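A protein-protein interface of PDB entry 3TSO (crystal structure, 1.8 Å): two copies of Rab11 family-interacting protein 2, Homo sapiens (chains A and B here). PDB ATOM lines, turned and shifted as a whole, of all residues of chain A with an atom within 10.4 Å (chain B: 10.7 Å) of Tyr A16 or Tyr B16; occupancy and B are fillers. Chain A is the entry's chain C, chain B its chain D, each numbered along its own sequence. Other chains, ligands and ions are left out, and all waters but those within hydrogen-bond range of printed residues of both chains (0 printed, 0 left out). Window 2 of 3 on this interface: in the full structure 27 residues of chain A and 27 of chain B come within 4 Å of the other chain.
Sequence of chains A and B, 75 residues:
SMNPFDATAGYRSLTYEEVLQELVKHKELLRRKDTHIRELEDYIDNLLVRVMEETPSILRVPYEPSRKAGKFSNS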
ATOM      1  N   ARG A  12      20.872   7.756 -12.010  1.00  0.00           N
ATOM      2  CA  ARG A  12      21.419   8.042 -13.387  1.00  0.00           C
ATOM      3  C   ARG A  12      20.296   7.995 -14.431  1.00  0.00           C
ATOM      4  O   ARG A  12      19.268   7.366 -14.222  1.00  0.00           O
ATOM      5  CB  ARG A  12      22.615   7.144 -13.766  1.00  0.00           C
ATOM      6  CG  ARG A  12      22.241   5.731 -14.207  1.00  0.00           C
ATOM      7  CD  ARG A  12      23.026   5.268 -15.437  1.00  0.00           C
ATOM      8  NE  ARG A  12      22.859   3.830 -15.679  1.00  0.00           N
ATOM      9  CZ  ARG A  12      22.039   3.290 -16.583  1.00  0.00           C
ATOM     10  NH1 ARG A  12      21.289   4.059 -17.346  1.00  0.00           N
ATOM     11  NH2 ARG A  12      21.964   1.967 -16.717  1.00  0.00           N
ATOM     12  N   SER A  13      20.503   8.712 -15.533  1.00  0.00           N
ATOM     13  CA  SER A  13      19.551   8.755 -16.638  1.00  0.00           C
ATOM     14  C   SER A  13      19.274   7.381 -17.311  1.00  0.00           C
ATOM     15  O   SER A  13      20.177   6.710 -17.782  1.00  0.00           O
ATOM     16  CB  SER A  13      20.104   9.746 -17.668  1.00  0.00           C
ATOM     17  OG  SER A  13      19.133  10.097 -18.613  1.00  0.00           O
ATOM     18  N   LEU A  14      18.010   6.993 -17.418  1.00  0.00           N
ATOM     19  CA  LEU A  14      17.670   5.702 -18.027  1.00  0.00           C
ATOM     20  C   LEU A  14      17.640   5.851 -19.522  1.00  0.00           C
ATOM     21  O   LEU A  14      17.155   6.854 -20.057  1.00  0.00           O
ATOM     22  CB  LEU A  14      16.282   5.212 -17.602  1.00  0.00           C
ATOM     23  CG  LEU A  14      15.984   4.706 -16.195  1.00  0.00           C
ATOM     24  CD1 LEU A  14      14.685   3.846 -16.331  1.00  0.00           C
ATOM     25  CD2 LEU A  14      17.097   3.923 -15.703  1.00  0.00           C
ATOM     26  N   THR A  15      18.119   4.824 -20.195  1.00  0.00           N
ATOM     27  CA  THR A  15      18.102   4.825 -21.619  1.00  0.00           C
ATOM     28  C   THR A  15      16.699   4.571 -22.081  1.00  0.00           C
ATOM     29  O   THR A  15      15.821   4.175 -21.269  1.00  0.00           O
ATOM     30  CB  THR A  15      18.988   3.720 -22.156  1.00  0.00           C
ATOM     31  OG1 THR A  15      18.438   2.438 -21.757  1.00  0.00           O
ATOM     32  CG2 THR A  15      20.402   3.846 -21.566  1.00  0.00           C
ATOM     33  N   TYR A  16      16.513   4.656 -23.397  1.00  0.00           N
ATOM     34  CA  TYR A  16      15.196   4.490 -23.986  1.00  0.00           C
ATOM     35  C   TYR A  16      14.758   3.074 -23.663  1.00  0.00           C
ATOM     36  O   TYR A  16      13.603   2.843 -23.252  1.00  0.00           O
ATOM     37  CB  TYR A  16      15.270   4.649 -25.480  1.00  0.00           C
ATOM     38  CG  TYR A  16      13.953   4.501 -26.234  1.00  0.00           C
ATOM     39  CD1 TYR A  16      13.454   3.242 -26.554  1.00  0.00           C
ATOM     40  CD2 TYR A  16      13.223   5.641 -26.637  1.00  0.00           C
ATOM     41  CE1 TYR A  16      12.284   3.070 -27.272  1.00  0.00           C
ATOM     42  CE2 TYR A  16      12.027   5.489 -27.384  1.00  0.00           C
ATOM     43  CZ  TYR A  16      11.558   4.212 -27.658  1.00  0.00           C
ATOM     44  OH  TYR A  16      10.400   4.070 -28.393  1.00  0.00           O
ATOM     45  N   GLU A  17      15.685   2.133 -23.864  1.00  0.00           N
ATOM     46  CA  GLU A  17      15.359   0.749 -23.664  1.00  0.00           C
ATOM     47  C   GLU A  17      15.090   0.412 -22.219  1.00  0.00           C
ATOM     48  O   GLU A  17      14.256  -0.448 -21.956  1.00  0.00           O
ATOM     49  CB  GLU A  17      16.414  -0.153 -24.282  1.00  0.00           C
ATOM     50  CG  GLU A  17      16.199  -0.223 -25.839  1.00  0.00           C
ATOM     51  CD  GLU A  17      17.353  -0.906 -26.580  1.00  0.00           C
ATOM     52  OE1 GLU A  17      18.203  -1.533 -25.912  1.00  0.00           O
ATOM     53  OE2 GLU A  17      17.409  -0.833 -27.831  1.00  0.00           O
ATOM     54  N   GLU A  18      15.785   1.058 -21.283  1.00  0.00           N
ATOM     55  CA  GLU A  18      15.492   0.850 -19.909  1.00  0.00           C
ATOM     56  C   GLU A  18      14.090   1.369 -19.597  1.00  0.00           C
ATOM     57  O   GLU A  18      13.344   0.713 -18.895  1.00  0.00           O
ATOM     58  CB  GLU A  18      16.564   1.486 -19.019  1.00  0.00           C
ATOM     59  CG  GLU A  18      17.834   0.613 -19.069  1.00  0.00           C
ATOM     60  CD  GLU A  18      19.079   1.336 -18.622  1.00  0.00           C
ATOM     61  OE1 GLU A  18      19.013   2.586 -18.406  1.00  0.00           O
ATOM     62  OE2 GLU A  18      20.111   0.626 -18.434  1.00  0.00           O
ATOM     63  N   VAL A  19      13.727   2.537 -20.102  1.00  0.00           N
ATOM     64  CA  VAL A  19      12.352   3.071 -19.853  1.00  0.00           C
ATOM     65  C   VAL A  19      11.246   2.157 -20.458  1.00  0.00           C
ATOM     66  O   VAL A  19      10.193   1.875 -19.822  1.00  0.00           O
ATOM     67  CB  VAL A  19      12.248   4.489 -20.433  1.00  0.00           C
ATOM     68  CG1 VAL A  19      10.854   5.011 -20.252  1.00  0.00           C
ATOM     69  CG2 VAL A  19      13.221   5.424 -19.694  1.00  0.00           C
ATOM     70  N   LEU A  20      11.520   1.668 -21.661  1.00  0.00           N
ATOM     71  CA  LEU A  20      10.613   0.790 -22.405  1.00  0.00           C
ATOM     72  C   LEU A  20      10.468  -0.572 -21.731  1.00  0.00           C
ATOM     73  O   LEU A  20       9.376  -1.180 -21.768  1.00  0.00           O
ATOM     74  CB  LEU A  20      11.132   0.626 -23.822  1.00  0.00           C
ATOM     75  CG  LEU A  20      10.395  -0.264 -24.798  1.00  0.00           C
ATOM     76  CD1 LEU A  20      10.574  -1.725 -24.430  1.00  0.00           C
ATOM     77  CD2 LEU A  20       8.937   0.153 -24.783  1.00  0.00           C
ATOM     78  N   GLN A  21      11.545  -1.056 -21.112  1.00  0.00           N
ATOM     79  CA  GLN A  21      11.440  -2.313 -20.320  1.00  0.00           C
ATOM     80  C   GLN A  21      10.539  -2.098 -19.093  1.00  0.00           C
ATOM     81  O   GLN A  21       9.734  -2.969 -18.754  1.00  0.00           O
ATOM     82  CB  GLN A  21      12.798  -2.897 -19.910  1.00  0.00           C
ATOM     83  CG  GLN A  21      13.530  -3.604 -21.042  1.00  0.00           C
ATOM     84  N   GLU A  22      10.684  -0.947 -18.446  1.00  0.00           N
ATOM     85  CA  GLU A  22       9.890  -0.622 -17.261  1.00  0.00           C
ATOM     86  C   GLU A  22       8.398  -0.527 -17.648  1.00  0.00           C
ATOM     87  O   GLU A  22       7.497  -1.035 -16.926  1.00  0.00           O
ATOM     88  CB  GLU A  22      10.461   0.638 -16.529  1.00  0.00           C
ATOM     89  CG  GLU A  22      11.521   0.344 -15.488  1.00  0.00           C
ATOM     90  CD  GLU A  22      11.015  -0.521 -14.334  1.00  0.00           C
ATOM     91  OE1 GLU A  22      11.407  -1.694 -14.283  1.00  0.00           O
ATOM     92  OE2 GLU A  22      10.198  -0.055 -13.503  1.00  0.00           O
ATOM     93  N   LEU A  23       8.140   0.027 -18.825  1.00  0.00           N
ATOM     94  CA  LEU A  23       6.782   0.171 -19.303  1.00  0.00           C
ATOM     95  C   LEU A  23       6.207  -1.227 -19.556  1.00  0.00           C
ATOM     96  O   LEU A  23       5.121  -1.545 -19.067  1.00  0.00           O
ATOM     97  CB  LEU A  23       6.765   0.921 -20.621  1.00  0.00           C
ATOM     98  CG  LEU A  23       5.525   1.651 -21.117  1.00  0.00           C
ATOM     99  CD1 LEU A  23       5.443   1.884 -22.643  1.00  0.00           C
ATOM    100  CD2 LEU A  23       4.150   1.409 -20.437  1.00  0.00           C
ATOM    101  N   VAL A  24       6.969  -2.064 -20.266  1.00  0.00           N
ATOM    102  CA  VAL A  24       6.548  -3.459 -20.508  1.00  0.00           C
ATOM    103  C   VAL A  24       6.275  -4.198 -19.179  1.00  0.00           C
ATOM    104  O   VAL A  24       5.229  -4.894 -19.003  1.00  0.00           O
ATOM    105  CB  VAL A  24       7.594  -4.207 -21.397  1.00  0.00           C
ATOM    106  CG1 VAL A  24       7.351  -5.734 -21.382  1.00  0.00           C
ATOM    107  CG2 VAL A  24       7.543  -3.649 -22.846  1.00  0.00           C
ATOM    108  N   ARG B  12       3.423   4.190 -35.183  1.00  0.00           N
ATOM    109  CA  ARG B  12       4.360   5.354 -34.977  1.00  0.00           C
ATOM    110  C   ARG B  12       5.425   5.047 -33.908  1.00  0.00           C
ATOM    111  O   ARG B  12       5.111   4.548 -32.821  1.00  0.00           O
ATOM    112  CB  ARG B  12       3.596   6.623 -34.589  1.00  0.00           C
ATOM    113  N   SER B  13       6.683   5.347 -34.218  1.00  0.00           N
ATOM    114  CA  SER B  13       7.763   5.044 -33.282  1.00  0.00           C
ATOM    115  C   SER B  13       7.714   6.063 -32.169  1.00  0.00           C
ATOM    116  O   SER B  13       8.082   7.216 -32.386  1.00  0.00           O
ATOM    117  CB  SER B  13       9.141   5.133 -33.956  1.00  0.00           C
ATOM    118  OG  SER B  13      10.077   4.320 -33.250  1.00  0.00           O
ATOM    119  N   LEU B  14       7.278   5.646 -30.988  1.00  0.00           N
ATOM    120  CA  LEU B  14       7.198   6.570 -29.857  1.00  0.00           C
ATOM    121  C   LEU B  14       8.580   7.120 -29.473  1.00  0.00           C
ATOM    122  O   LEU B  14       9.566   6.378 -29.485  1.00  0.00           O
ATOM    123  CB  LEU B  14       6.568   5.866 -28.656  1.00  0.00           C
ATOM    124  CG  LEU B  14       5.121   5.393 -28.786  1.00  0.00           C
ATOM    125  CD1 LEU B  14       4.560   5.120 -27.405  1.00  0.00           C
ATOM    126  CD2 LEU B  14       4.307   6.483 -29.472  1.00  0.00           C
ATOM    127  N   THR B  15       8.621   8.406 -29.149  1.00  0.00           N
ATOM    128  CA  THR B  15       9.828   9.079 -28.654  1.00  0.00           C
ATOM    129  C   THR B  15      10.085   8.696 -27.203  1.00  0.00           C
ATOM    130  O   THR B  15       9.216   8.135 -26.530  1.00  0.00           O
ATOM    131  CB  THR B  15       9.686  10.582 -28.735  1.00  0.00           C
ATOM    132  OG1 THR B  15       8.793  11.007 -27.718  1.00  0.00           O
ATOM    133  CG2 THR B  15       9.187  11.057 -30.197  1.00  0.00           C
ATOM    134  N   TYR B  16      11.275   8.993 -26.701  1.00  0.00           N
ATOM    135  CA  TYR B  16      11.603   8.760 -25.289  1.00  0.00           C
ATOM    136  C   TYR B  16      10.583   9.384 -24.396  1.00  0.00           C
ATOM    137  O   TYR B  16      10.149   8.744 -23.424  1.00  0.00           O
ATOM    138  CB  TYR B  16      12.966   9.371 -24.950  1.00  0.00           C
ATOM    139  CG  TYR B  16      13.487   9.089 -23.528  1.00  0.00           C
ATOM    140  CD1 TYR B  16      12.985   9.766 -22.429  1.00  0.00           C
ATOM    141  CD2 TYR B  16      14.490   8.162 -23.331  1.00  0.00           C
ATOM    142  CE1 TYR B  16      13.465   9.546 -21.159  1.00  0.00           C
ATOM    143  CE2 TYR B  16      14.981   7.899 -22.084  1.00  0.00           C
ATOM    144  CZ  TYR B  16      14.492   8.598 -21.002  1.00  0.00           C
ATOM    145  OH  TYR B  16      15.004   8.350 -19.784  1.00  0.00           O
ATOM    146  N   GLU B  17      10.218  10.639 -24.667  1.00  0.00           N
ATOM    147  CA  GLU B  17       9.248  11.315 -23.820  1.00  0.00           C
ATOM    148  C   GLU B  17       7.827  10.696 -23.837  1.00  0.00           C
ATOM    149  O   GLU B  17       7.138  10.624 -22.808  1.00  0.00           O
ATOM    150  CB  GLU B  17       9.163  12.781 -24.174  1.00  0.00           C
ATOM    151  CG  GLU B  17      10.286  13.620 -23.471  1.00  0.00           C
ATOM    152  CD  GLU B  17      10.444  14.981 -24.118  1.00  0.00           C
ATOM    153  OE1 GLU B  17       9.446  15.485 -24.678  1.00  0.00           O
ATOM    154  OE2 GLU B  17      11.565  15.520 -24.085  1.00  0.00           O
ATOM    155  N   GLU B  18       7.427  10.229 -24.987  1.00  0.00           N
ATOM    156  CA  GLU B  18       6.148   9.526 -25.104  1.00  0.00           C
ATOM    157  C   GLU B  18       6.149   8.208 -24.335  1.00  0.00           C
ATOM    158  O   GLU B  18       5.122   7.841 -23.751  1.00  0.00           O
ATOM    159  CB  GLU B  18       5.801   9.275 -26.585  1.00  0.00           C
ATOM    160  CG  GLU B  18       5.488  10.554 -27.345  1.00  0.00           C
ATOM    161  CD  GLU B  18       5.314  10.345 -28.818  1.00  0.00           C
ATOM    162  OE1 GLU B  18       5.965   9.463 -29.447  1.00  0.00           O
ATOM    163  OE2 GLU B  18       4.482  11.095 -29.364  1.00  0.00           O
ATOM    164  N   VAL B  19       7.268   7.477 -24.356  1.00  0.00           N
ATOM    165  CA  VAL B  19       7.388   6.228 -23.564  1.00  0.00           C
ATOM    166  C   VAL B  19       7.334   6.522 -22.080  1.00  0.00           C
ATOM    167  O   VAL B  19       6.594   5.867 -21.330  1.00  0.00           O
ATOM    168  CB  VAL B  19       8.673   5.375 -23.908  1.00  0.00           C
ATOM    169  CG1 VAL B  19       8.725   4.062 -23.070  1.00  0.00           C
ATOM    170  CG2 VAL B  19       8.710   5.075 -25.435  1.00  0.00           C
ATOM    171  N   LEU B  20       8.093   7.514 -21.648  1.00  0.00           N
ATOM    172  CA  LEU B  20       8.169   7.854 -20.285  1.00  0.00           C
ATOM    173  C   LEU B  20       6.799   8.305 -19.775  1.00  0.00           C
ATOM    174  O   LEU B  20       6.407   7.989 -18.634  1.00  0.00           O
ATOM    175  CB  LEU B  20       9.197   8.991 -20.108  1.00  0.00           C
ATOM    176  CG  LEU B  20       9.336   9.642 -18.742  1.00  0.00           C
ATOM    177  CD1 LEU B  20       9.602   8.594 -17.591  1.00  0.00           C
ATOM    178  CD2 LEU B  20      10.549  10.612 -18.813  1.00  0.00           C
ATOM    179  N   GLN B  21       6.067   9.033 -20.609  1.00  0.00           N
ATOM    180  CA  GLN B  21       4.732   9.517 -20.194  1.00  0.00           C
ATOM    181  C   GLN B  21       3.751   8.344 -19.997  1.00  0.00           C
ATOM    182  O   GLN B  21       2.995   8.328 -19.011  1.00  0.00           O
ATOM    183  CB  GLN B  21       4.160  10.526 -21.188  1.00  0.00           C
ATOM    184  CG  GLN B  21       4.678  11.957 -20.945  1.00  0.00           C
ATOM    185  N   GLU B  22       3.767   7.405 -20.951  1.00  0.00           N
ATOM    186  CA  GLU B  22       3.057   6.134 -20.839  1.00  0.00           C
ATOM    187  C   GLU B  22       3.484   5.378 -19.546  1.00  0.00           C
ATOM    188  O   GLU B  22       2.614   4.904 -18.775  1.00  0.00           O
ATOM    189  CB  GLU B  22       3.274   5.303 -22.114  1.00  0.00           C
ATOM    190  CG  GLU B  22       2.224   4.231 -22.389  1.00  0.00           C
ATOM    191  CD  GLU B  22       0.766   4.765 -22.476  1.00  0.00           C
ATOM    192  OE1 GLU B  22       0.541   5.953 -22.775  1.00  0.00           O
ATOM    193  OE2 GLU B  22      -0.157   3.975 -22.228  1.00  0.00           O
ATOM    194  N   LEU B  23       4.788   5.311 -19.253  1.00  0.00           N
ATOM    195  CA  LEU B  23       5.238   4.725 -17.983  1.00  0.00           C
ATOM    196  C   LEU B  23       4.683   5.414 -16.747  1.00  0.00           C
ATOM    197  O   LEU B  23       4.167   4.728 -15.847  1.00  0.00           O
ATOM    198  CB  LEU B  23       6.762   4.704 -17.873  1.00  0.00           C
ATOM    199  CG  LEU B  23       7.519   3.612 -17.131  1.00  0.00           C
ATOM    200  CD1 LEU B  23       8.779   4.157 -16.467  1.00  0.00           C
ATOM    201  CD2 LEU B  23       6.730   2.661 -16.199  1.00  0.00           C
ATOM    202  N   VAL B  24       4.823   6.757 -16.671  1.00  0.00           N
ATOM    203  CA  VAL B  24       4.301   7.546 -15.513  1.00  0.00           C
ATOM    204  C   VAL B  24       2.807   7.263 -15.349  1.00  0.00           C
ATOM    205  O   VAL B  24       2.331   7.067 -14.240  1.00  0.00           O
ATOM    206  CB  VAL B  24       4.588   9.088 -15.705  1.00  0.00           C
ATOM    207  CG1 VAL B  24       3.774   9.951 -14.777  1.00  0.00           C
ATOM    208  CG2 VAL B  24       6.069   9.377 -15.582  1.00  0.00           C
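The side-chain hydroxyl (OH) of Tyr B16 sits at hydrogen-bond distance from the backbone carbonyl oxygen (O) of Leu A14. The side-chain hydroxyl (OH) of Tyr A16 sits at hydrogen-bond distance from the backbone carbonyl oxygen (O) of Leu B14.
The side-chain hydroxyl of Thr B15 sits close to the backbone NH of Glu B17, 3.4 Å away. The backbone NH (N) of Thr A15 sits at hydrogen-bond distance from the side-chain carboxylate (OE1) of Glu A18 (3.0 Å). OG1 of Thr A15 sits close to N of Glu A17 (3.5 Å). The backbone NH (N) of Thr B15 lies within hydrogen-bond range of the side-chain carboxylate (OE1) of Glu B18, 2.9 Å away.
CE2 of Tyr A16 touches C of Thr B15, 3.8 Å away. Tyr B16 touches Tyr A16. Val B19 touches Tyr A16. Tyr B16 touches Val A19 (OH to CG2, 3.4 Å). CG1 of Val B19 touches CG1 of Val A19 (3.7 Å). Leu B20 touches Val A19. Val B19 touches Leu A20 (CG1 to CA, 3.8 Å). Leu B23 touches Glu A22. Glu B22 touches Leu A23 (CG to CD2, 3.9 Å). N of Leu A23 touches CD2 of Leu B23 (3.98 Å).
Tyr A16 touches four residues of chain B. Of chain A, only Leu A14 (2.6 Å), Thr A15 (3.7 Å), Tyr A16 (3.6 Å) and Val A19 (3.4 Å) come within 4 Å of Tyr B16. Of chain B, only Tyr B16 (3.7 Å) comes within 4 Å of Thr A15. No residue of chain B comes within 4 Å of Glu A17. Val A19 touches just these residues of chain B: Tyr B16, Val B19 and Leu B20. Of the printed residues of chain A, Thr B15 touches Tyr A16. Of the printed residues of chain A, Leu B23 touches Glu A22 (3.8 Å) and Leu A23 (3.98 Å). Printed residues of chain B within 4 Å of Leu A23: Val B19 (3.96 Å), Glu B22 (3.9 Å) and Leu B23 (3.98 Å). Of the printed residues of chain B, Leu A20 touches Val B19. Printed residues of chain A within 4 Å of Leu B14: Tyr A16 (2.7 Å). Val A24 touches none of the printed residues of chain B. Glu A18 touches none of the printed residues of chain B. The nearest residue of chain A that does not touch Tyr B16 is Ser A13 (4.6 Å). The nearest printed residue of chain B that does not touch Leu A23 is Leu B14 (5.8 Å).
Of the 13 printed residues of chain B, 7 touch a printed residue of chain A. Hydrophobic or aromatic side chains of chain B that line the printed part of chain A: Tyr B16, Val B19 and Leu B23. Along chain B the printed residues that touch a printed residue of chain A span positions 14 to 23. Among the printed residues, no Asp or Glu carboxylate lies within 4 Å of a Lys or Arg side-chain nitrogen of the other chain.
Leu A14 touches Tyr B16, and with the chains exchanged Tyr A16 touches Leu B14. Thr A15 touches Tyr B16, and with the chains exchanged Tyr A16 touches Thr B15. Val B19 touches its own counterpart, Val A19. Glu A22 touches Leu B23, and with the chains exchanged Leu A23 touches Glu B22. Positions printed for both chains: 12, 13, 14, 15, 16, 17, 18, 19, 20, 21, 22, 23 and 24. Of the 14 pairs that touch across the chains among the printed residues, 13 have their exchanged pair printed and touching as well.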
